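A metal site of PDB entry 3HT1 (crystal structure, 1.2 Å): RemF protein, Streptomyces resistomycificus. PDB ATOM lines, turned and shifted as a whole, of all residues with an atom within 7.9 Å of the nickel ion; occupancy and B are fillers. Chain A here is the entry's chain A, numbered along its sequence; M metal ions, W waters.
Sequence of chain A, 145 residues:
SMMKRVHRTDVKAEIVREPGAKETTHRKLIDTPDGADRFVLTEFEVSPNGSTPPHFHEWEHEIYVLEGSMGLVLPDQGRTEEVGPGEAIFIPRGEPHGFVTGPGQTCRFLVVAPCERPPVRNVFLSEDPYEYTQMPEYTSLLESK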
ATOM      1  N   GLU A  18      -4.521   8.707  -1.487  1.00  0.00           N
ATOM      2  CA  GLU A  18      -5.682   7.938  -1.047  1.00  0.00           C
ATOM      3  C   GLU A  18      -6.282   7.197  -2.236  1.00  0.00           C
ATOM      4  O   GLU A  18      -6.646   7.845  -3.221  1.00  0.00           O
ATOM      5  CB  GLU A  18      -6.708   8.848  -0.397  1.00  0.00           C
ATOM      6  CG  GLU A  18      -7.880   8.079   0.150  1.00  0.00           C
ATOM      7  CD  GLU A  18      -8.877   8.845   0.992  1.00  0.00           C
ATOM      8  OE1 GLU A  18      -9.045  10.085   0.762  1.00  0.00           O
ATOM      9  OE2 GLU A  18      -9.567   8.223   1.856  1.00  0.00           O
ATOM     10  N   THR A  52     -13.167  12.432  -3.448  1.00  0.00           N
ATOM     11  CA  THR A  52     -12.442  11.574  -2.543  1.00  0.00           C
ATOM     12  C   THR A  52     -13.432  10.581  -1.926  1.00  0.00           C
ATOM     13  O   THR A  52     -14.614  10.859  -1.713  1.00  0.00           O
ATOM     14  CB  THR A  52     -11.711  12.389  -1.469  1.00  0.00           C
ATOM     15  OG1 THR A  52     -12.656  12.956  -0.599  1.00  0.00           O
ATOM     16  CG2 THR A  52     -10.909  13.516  -2.106  1.00  0.00           C
ATOM     17  N   PRO A  53     -12.962   9.348  -1.607  1.00  0.00           N
ATOM     18  CA  PRO A  53     -13.888   8.384  -1.039  1.00  0.00           C
ATOM     19  C   PRO A  53     -14.325   8.830   0.338  1.00  0.00           C
ATOM     20  O   PRO A  53     -13.469   9.147   1.179  1.00  0.00           O
ATOM     21  CB  PRO A  53     -13.046   7.090  -0.963  1.00  0.00           C
ATOM     22  CG  PRO A  53     -11.637   7.533  -1.044  1.00  0.00           C
ATOM     23  CD  PRO A  53     -11.631   8.821  -1.847  1.00  0.00           C
ATOM     24  N   PRO A  54     -15.595   8.880   0.640  1.00  0.00           N
ATOM     25  CA  PRO A  54     -15.973   9.316   1.992  1.00  0.00           C
ATOM     26  C   PRO A  54     -15.378   8.405   3.053  1.00  0.00           C
ATOM     27  O   PRO A  54     -15.308   7.189   2.893  1.00  0.00           O
ATOM     28  CB  PRO A  54     -17.512   9.230   1.955  1.00  0.00           C
ATOM     29  CG  PRO A  54     -17.824   9.549   0.513  1.00  0.00           C
ATOM     30  CD  PRO A  54     -16.776   8.767  -0.240  1.00  0.00           C
ATOM     31  N   HIS A  55     -14.857   8.999   4.118  1.00  0.00           N
ATOM     32  CA  HIS A  55     -14.126   8.228   5.100  1.00  0.00           C
ATOM     33  C   HIS A  55     -14.347   8.859   6.482  1.00  0.00           C
ATOM     34  O   HIS A  55     -14.919   9.950   6.606  1.00  0.00           O
ATOM     35  CB  HIS A  55     -12.654   8.189   4.677  1.00  0.00           C
ATOM     36  CG  HIS A  55     -11.851   9.445   4.717  1.00  0.00           C
ATOM     37  ND1 HIS A  55     -10.735   9.627   3.953  1.00  0.00           N
ATOM     38  CD2 HIS A  55     -11.922  10.587   5.466  1.00  0.00           C
ATOM     39  CE1 HIS A  55     -10.203  10.808   4.282  1.00  0.00           C
ATOM     40  NE2 HIS A  55     -10.900  11.429   5.177  1.00  0.00           N
ATOM     41  N   PHE A  56     -13.754   8.233   7.488  1.00  0.00           N
ATOM     42  CA  PHE A  56     -13.737   8.788   8.815  1.00  0.00           C
ATOM     43  C   PHE A  56     -12.431   8.350   9.475  1.00  0.00           C
ATOM     44  O   PHE A  56     -11.813   7.378   9.128  1.00  0.00           O
ATOM     45  CB  PHE A  56     -14.965   8.434   9.626  1.00  0.00           C
ATOM     46  CG  PHE A  56     -15.230   6.959   9.805  1.00  0.00           C
ATOM     47  CD1 PHE A  56     -15.799   6.198   8.810  1.00  0.00           C
ATOM     48  CD2 PHE A  56     -14.925   6.323  10.985  1.00  0.00           C
ATOM     49  CE1 PHE A  56     -16.095   4.873   8.995  1.00  0.00           C
ATOM     50  CE2 PHE A  56     -15.212   5.003  11.184  1.00  0.00           C
ATOM     51  CZ  PHE A  56     -15.776   4.229  10.191  1.00  0.00           C
ATOM     52  N   HIS A  57     -12.047   9.138  10.510  1.00  0.00           N
ATOM     53  CA  HIS A  57     -10.754   8.859  11.125  1.00  0.00           C
ATOM     54  C   HIS A  57     -10.668   9.533  12.494  1.00  0.00           C
ATOM     55  O   HIS A  57     -11.298  10.558  12.728  1.00  0.00           O
ATOM     56  CB  HIS A  57      -9.601   9.337  10.250  1.00  0.00           C
ATOM     57  CG  HIS A  57      -9.804  10.632   9.545  1.00  0.00           C
ATOM     58  ND1 HIS A  57      -9.694  11.860  10.094  1.00  0.00           N
ATOM     59  CD2 HIS A  57     -10.075  10.882   8.231  1.00  0.00           C
ATOM     60  CE1 HIS A  57      -9.902  12.781   9.175  1.00  0.00           C
ATOM     61  NE2 HIS A  57     -10.144  12.246   7.986  1.00  0.00           N
ATOM     62  N   TRP A  59      -8.903  11.627  13.963  1.00  0.00           N
ATOM     63  CA  TRP A  59      -8.165  12.882  13.958  1.00  0.00           C
ATOM     64  C   TRP A  59      -9.081  13.910  13.293  1.00  0.00           C
ATOM     65  O   TRP A  59      -9.652  13.613  12.247  1.00  0.00           O
ATOM     66  CB  TRP A  59      -6.823  12.737  13.291  1.00  0.00           C
ATOM     67  CG  TRP A  59      -6.598  12.048  11.993  1.00  0.00           C
ATOM     68  CD1 TRP A  59      -6.520  10.687  11.811  1.00  0.00           C
ATOM     69  CD2 TRP A  59      -6.396  12.615  10.689  1.00  0.00           C
ATOM     70  NE1 TRP A  59      -6.290  10.368  10.493  1.00  0.00           N
ATOM     71  CE2 TRP A  59      -6.204  11.545   9.774  1.00  0.00           C
ATOM     72  CE3 TRP A  59      -6.350  13.939  10.196  1.00  0.00           C
ATOM     73  CZ2 TRP A  59      -5.988  11.797   8.422  1.00  0.00           C
ATOM     74  CZ3 TRP A  59      -6.122  14.164   8.833  1.00  0.00           C
ATOM     75  CH2 TRP A  59      -5.937  13.083   7.990  1.00  0.00           C
ATOM     76  N   GLU A  60      -9.191  15.043  13.907  1.00  0.00           N
ATOM     77  CA  GLU A  60     -10.048  16.113  13.475  1.00  0.00           C
ATOM     78  C   GLU A  60      -9.439  16.849  12.270  1.00  0.00           C
ATOM     79  O   GLU A  60      -8.229  16.889  12.106  1.00  0.00           O
ATOM     80  CB  GLU A  60     -10.288  17.066  14.627  1.00  0.00           C
ATOM     81  CG  GLU A  60      -9.099  17.775  15.217  1.00  0.00           C
ATOM     82  CD  GLU A  60      -8.329  17.040  16.303  1.00  0.00           C
ATOM     83  OE1 GLU A  60      -8.390  15.776  16.342  1.00  0.00           O
ATOM     84  OE2 GLU A  60      -7.624  17.712  17.084  1.00  0.00           O
ATOM     85  N   HIS A  61     -10.317  17.453  11.469  1.00  0.00           N
ATOM     86  CA  HIS A  61      -9.934  18.390  10.436  1.00  0.00           C
ATOM     87  C   HIS A  61     -10.351  19.809  10.769  1.00  0.00           C
ATOM     88  O   HIS A  61     -11.455  20.007  11.284  1.00  0.00           O
ATOM     89  CB  HIS A  61     -10.576  18.105   9.073  1.00  0.00           C
ATOM     90  CG  HIS A  61     -10.158  16.911   8.328  1.00  0.00           C
ATOM     91  ND1 HIS A  61      -8.857  16.584   8.053  1.00  0.00           N
ATOM     92  CD2 HIS A  61     -10.878  15.919   7.711  1.00  0.00           C
ATOM     93  CE1 HIS A  61      -8.825  15.482   7.319  1.00  0.00           C
ATOM     94  NE2 HIS A  61     -10.021  15.024   7.075  1.00  0.00           N
ATOM     95  N   ILE A  63     -10.489  23.169   8.365  1.00  0.00           N
ATOM     96  CA  ILE A  63     -10.426  23.501   6.943  1.00  0.00           C
ATOM     97  C   ILE A  63     -10.748  24.948   6.737  1.00  0.00           C
ATOM     98  O   ILE A  63     -11.649  25.487   7.391  1.00  0.00           O
ATOM     99  CB  ILE A  63     -11.391  22.596   6.160  1.00  0.00           C
ATOM    100  CG1 ILE A  63     -10.926  21.119   6.245  1.00  0.00           C
ATOM    101  CG2 ILE A  63     -11.599  23.031   4.746  1.00  0.00           C
ATOM    102  CD1 ILE A  63     -11.998  20.135   5.864  1.00  0.00           C
ATOM    103  N   ILE A  91     -14.309  19.409  11.388  1.00  0.00           N
ATOM    104  CA  ILE A  91     -14.828  18.047  11.255  1.00  0.00           C
ATOM    105  C   ILE A  91     -14.256  17.268  12.423  1.00  0.00           C
ATOM    106  O   ILE A  91     -13.051  16.990  12.474  1.00  0.00           O
ATOM    107  CB  ILE A  91     -14.467  17.396   9.916  1.00  0.00           C
ATOM    108  CG1 ILE A  91     -14.897  18.251   8.760  1.00  0.00           C
ATOM    109  CG2 ILE A  91     -15.133  16.023   9.835  1.00  0.00           C
ATOM    110  CD1 ILE A  91     -14.606  17.739   7.405  1.00  0.00           C
ATOM    111  N   GLU A  95     -16.284  11.784  12.380  1.00  0.00           N
ATOM    112  CA  GLU A  95     -17.411  12.209  11.536  1.00  0.00           C
ATOM    113  C   GLU A  95     -17.117  11.842  10.097  1.00  0.00           C
ATOM    114  O   GLU A  95     -16.077  12.257   9.571  1.00  0.00           O
ATOM    115  CB  GLU A  95     -17.676  13.703  11.684  1.00  0.00           C
ATOM    116  CG  GLU A  95     -18.878  14.125  10.823  1.00  0.00           C
ATOM    117  CD  GLU A  95     -20.230  13.754  11.340  1.00  0.00           C
ATOM    118  OE1 GLU A  95     -20.356  13.519  12.558  1.00  0.00           O
ATOM    119  OE2 GLU A  95     -21.189  13.734  10.509  1.00  0.00           O
ATOM    120  N   PRO A  96     -17.971  11.086   9.403  1.00  0.00           N
ATOM    121  CA  PRO A  96     -17.692  10.756   7.995  1.00  0.00           C
ATOM    122  C   PRO A  96     -17.779  11.955   7.090  1.00  0.00           C
ATOM    123  O   PRO A  96     -18.604  12.849   7.237  1.00  0.00           O
ATOM    124  CB  PRO A  96     -18.780   9.710   7.676  1.00  0.00           C
ATOM    125  CG  PRO A  96     -19.188   9.166   8.998  1.00  0.00           C
ATOM    126  CD  PRO A  96     -19.158  10.353   9.917  1.00  0.00           C
ATOM    127  N   HIS A  97     -16.899  12.001   6.081  1.00  0.00           N
ATOM    128  CA  HIS A  97     -16.813  13.126   5.168  1.00  0.00           C
ATOM    129  C   HIS A  97     -16.065  12.740   3.904  1.00  0.00           C
ATOM    130  O   HIS A  97     -15.176  11.874   3.899  1.00  0.00           O
ATOM    131  CB  HIS A  97     -16.079  14.317   5.866  1.00  0.00           C
ATOM    132  CG  HIS A  97     -14.705  13.948   6.323  1.00  0.00           C
ATOM    133  ND1 HIS A  97     -14.480  13.246   7.492  1.00  0.00           N
ATOM    134  CD2 HIS A  97     -13.473  14.116   5.771  1.00  0.00           C
ATOM    135  CE1 HIS A  97     -13.170  13.025   7.591  1.00  0.00           C
ATOM    136  NE2 HIS A  97     -12.529  13.532   6.566  1.00  0.00           N
ATOM    137  N   GLY A  98     -16.393  13.431   2.824  1.00  0.00           N
ATOM    138  CA  GLY A  98     -15.655  13.377   1.592  1.00  0.00           C
ATOM    139  C   GLY A  98     -15.858  14.695   0.814  1.00  0.00           C
ATOM    140  O   GLY A  98     -16.601  15.553   1.230  1.00  0.00           O
ATOM    141  N   PHE A  99     -15.202  14.810  -0.317  1.00  0.00           N
ATOM    142  CA  PHE A  99     -15.224  15.983  -1.146  1.00  0.00           C
ATOM    143  C   PHE A  99     -15.583  15.621  -2.554  1.00  0.00           C
ATOM    144  O   PHE A  99     -15.303  14.499  -3.020  1.00  0.00           O
ATOM    145  CB  PHE A  99     -13.884  16.743  -1.095  1.00  0.00           C
ATOM    146  CG  PHE A  99     -13.509  17.120   0.319  1.00  0.00           C
ATOM    147  CD1 PHE A  99     -14.034  18.230   0.919  1.00  0.00           C
ATOM    148  CD2 PHE A  99     -12.650  16.326   1.010  1.00  0.00           C
ATOM    149  CE1 PHE A  99     -13.716  18.562   2.215  1.00  0.00           C
ATOM    150  CE2 PHE A  99     -12.336  16.643   2.321  1.00  0.00           C
ATOM    151  CZ  PHE A  99     -12.877  17.766   2.898  1.00  0.00           C
ATOM    152  N   VAL A 111      -6.082  22.471   4.896  1.00  0.00           N
ATOM    153  CA  VAL A 111      -6.364  21.527   5.955  1.00  0.00           C
ATOM    154  C   VAL A 111      -5.263  21.600   6.999  1.00  0.00           C
ATOM    155  O   VAL A 111      -4.083  21.454   6.667  1.00  0.00           O
ATOM    156  CB  VAL A 111      -6.483  20.092   5.446  1.00  0.00           C
ATOM    157  CG1 VAL A 111      -6.697  19.117   6.603  1.00  0.00           C
ATOM    158  CG2 VAL A 111      -7.592  19.961   4.399  1.00  0.00           C
ATOM    159  N   VAL A 120      -7.318   6.048   8.046  1.00  0.00           N
ATOM    160  CA  VAL A 120      -8.691   6.339   7.710  1.00  0.00           C
ATOM    161  C   VAL A 120      -9.449   5.052   7.440  1.00  0.00           C
ATOM    162  O   VAL A 120      -8.892   4.020   7.069  1.00  0.00           O
ATOM    163  CB  VAL A 120      -8.871   7.321   6.531  1.00  0.00           C
ATOM    164  CG1 VAL A 120      -7.923   8.517   6.724  1.00  0.00           C
ATOM    165  CG2 VAL A 120      -8.685   6.672   5.185  1.00  0.00           C
HETATM  166 NI    NI M   1     -10.509  13.226   6.167  1.00  0.00          NI
HETATM  167  O   HOH W   1      -8.437  13.001   5.670  1.00  0.00           O
HETATM  168  O   HOH W   2     -10.689  14.203   4.312  1.00  0.00           O
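O of His 61 sits at hydrogen-bond distance from N of Ile 91 (2.9 Å).
A ring nitrogen (ND1) of His 97 lies within hydrogen-bond range of the backbone carbonyl oxygen (O) of Glu 95.
A ring nitrogen (ND1) of His 55 is in hydrogen-bond range of the side-chain carboxylate of Glu 18.
The backbone carbonyl oxygen (O) of Trp 59 lies within hydrogen-bond range of a ring nitrogen (ND1) of His 57 (2.8 Å).
NE2 of His 61 binds the nickel ion (2.1 Å).
NE2 of His 97 is bound to the nickel ion (2.1 Å).
NE2 of His 55 binds the nickel ion, 2.1 Å away.
The nickel ion is bound by a ring nitrogen (NE2) of His 57 (2.1 Å).
The nickel ion is bound by water W2 (2.1 Å).
Water W1 is bound to the nickel ion (2.1 Å).
The nickel ion has six donor atoms within binding distance.
Of the 19 residues printed, 4 come within 4 Å of the nickel ion.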
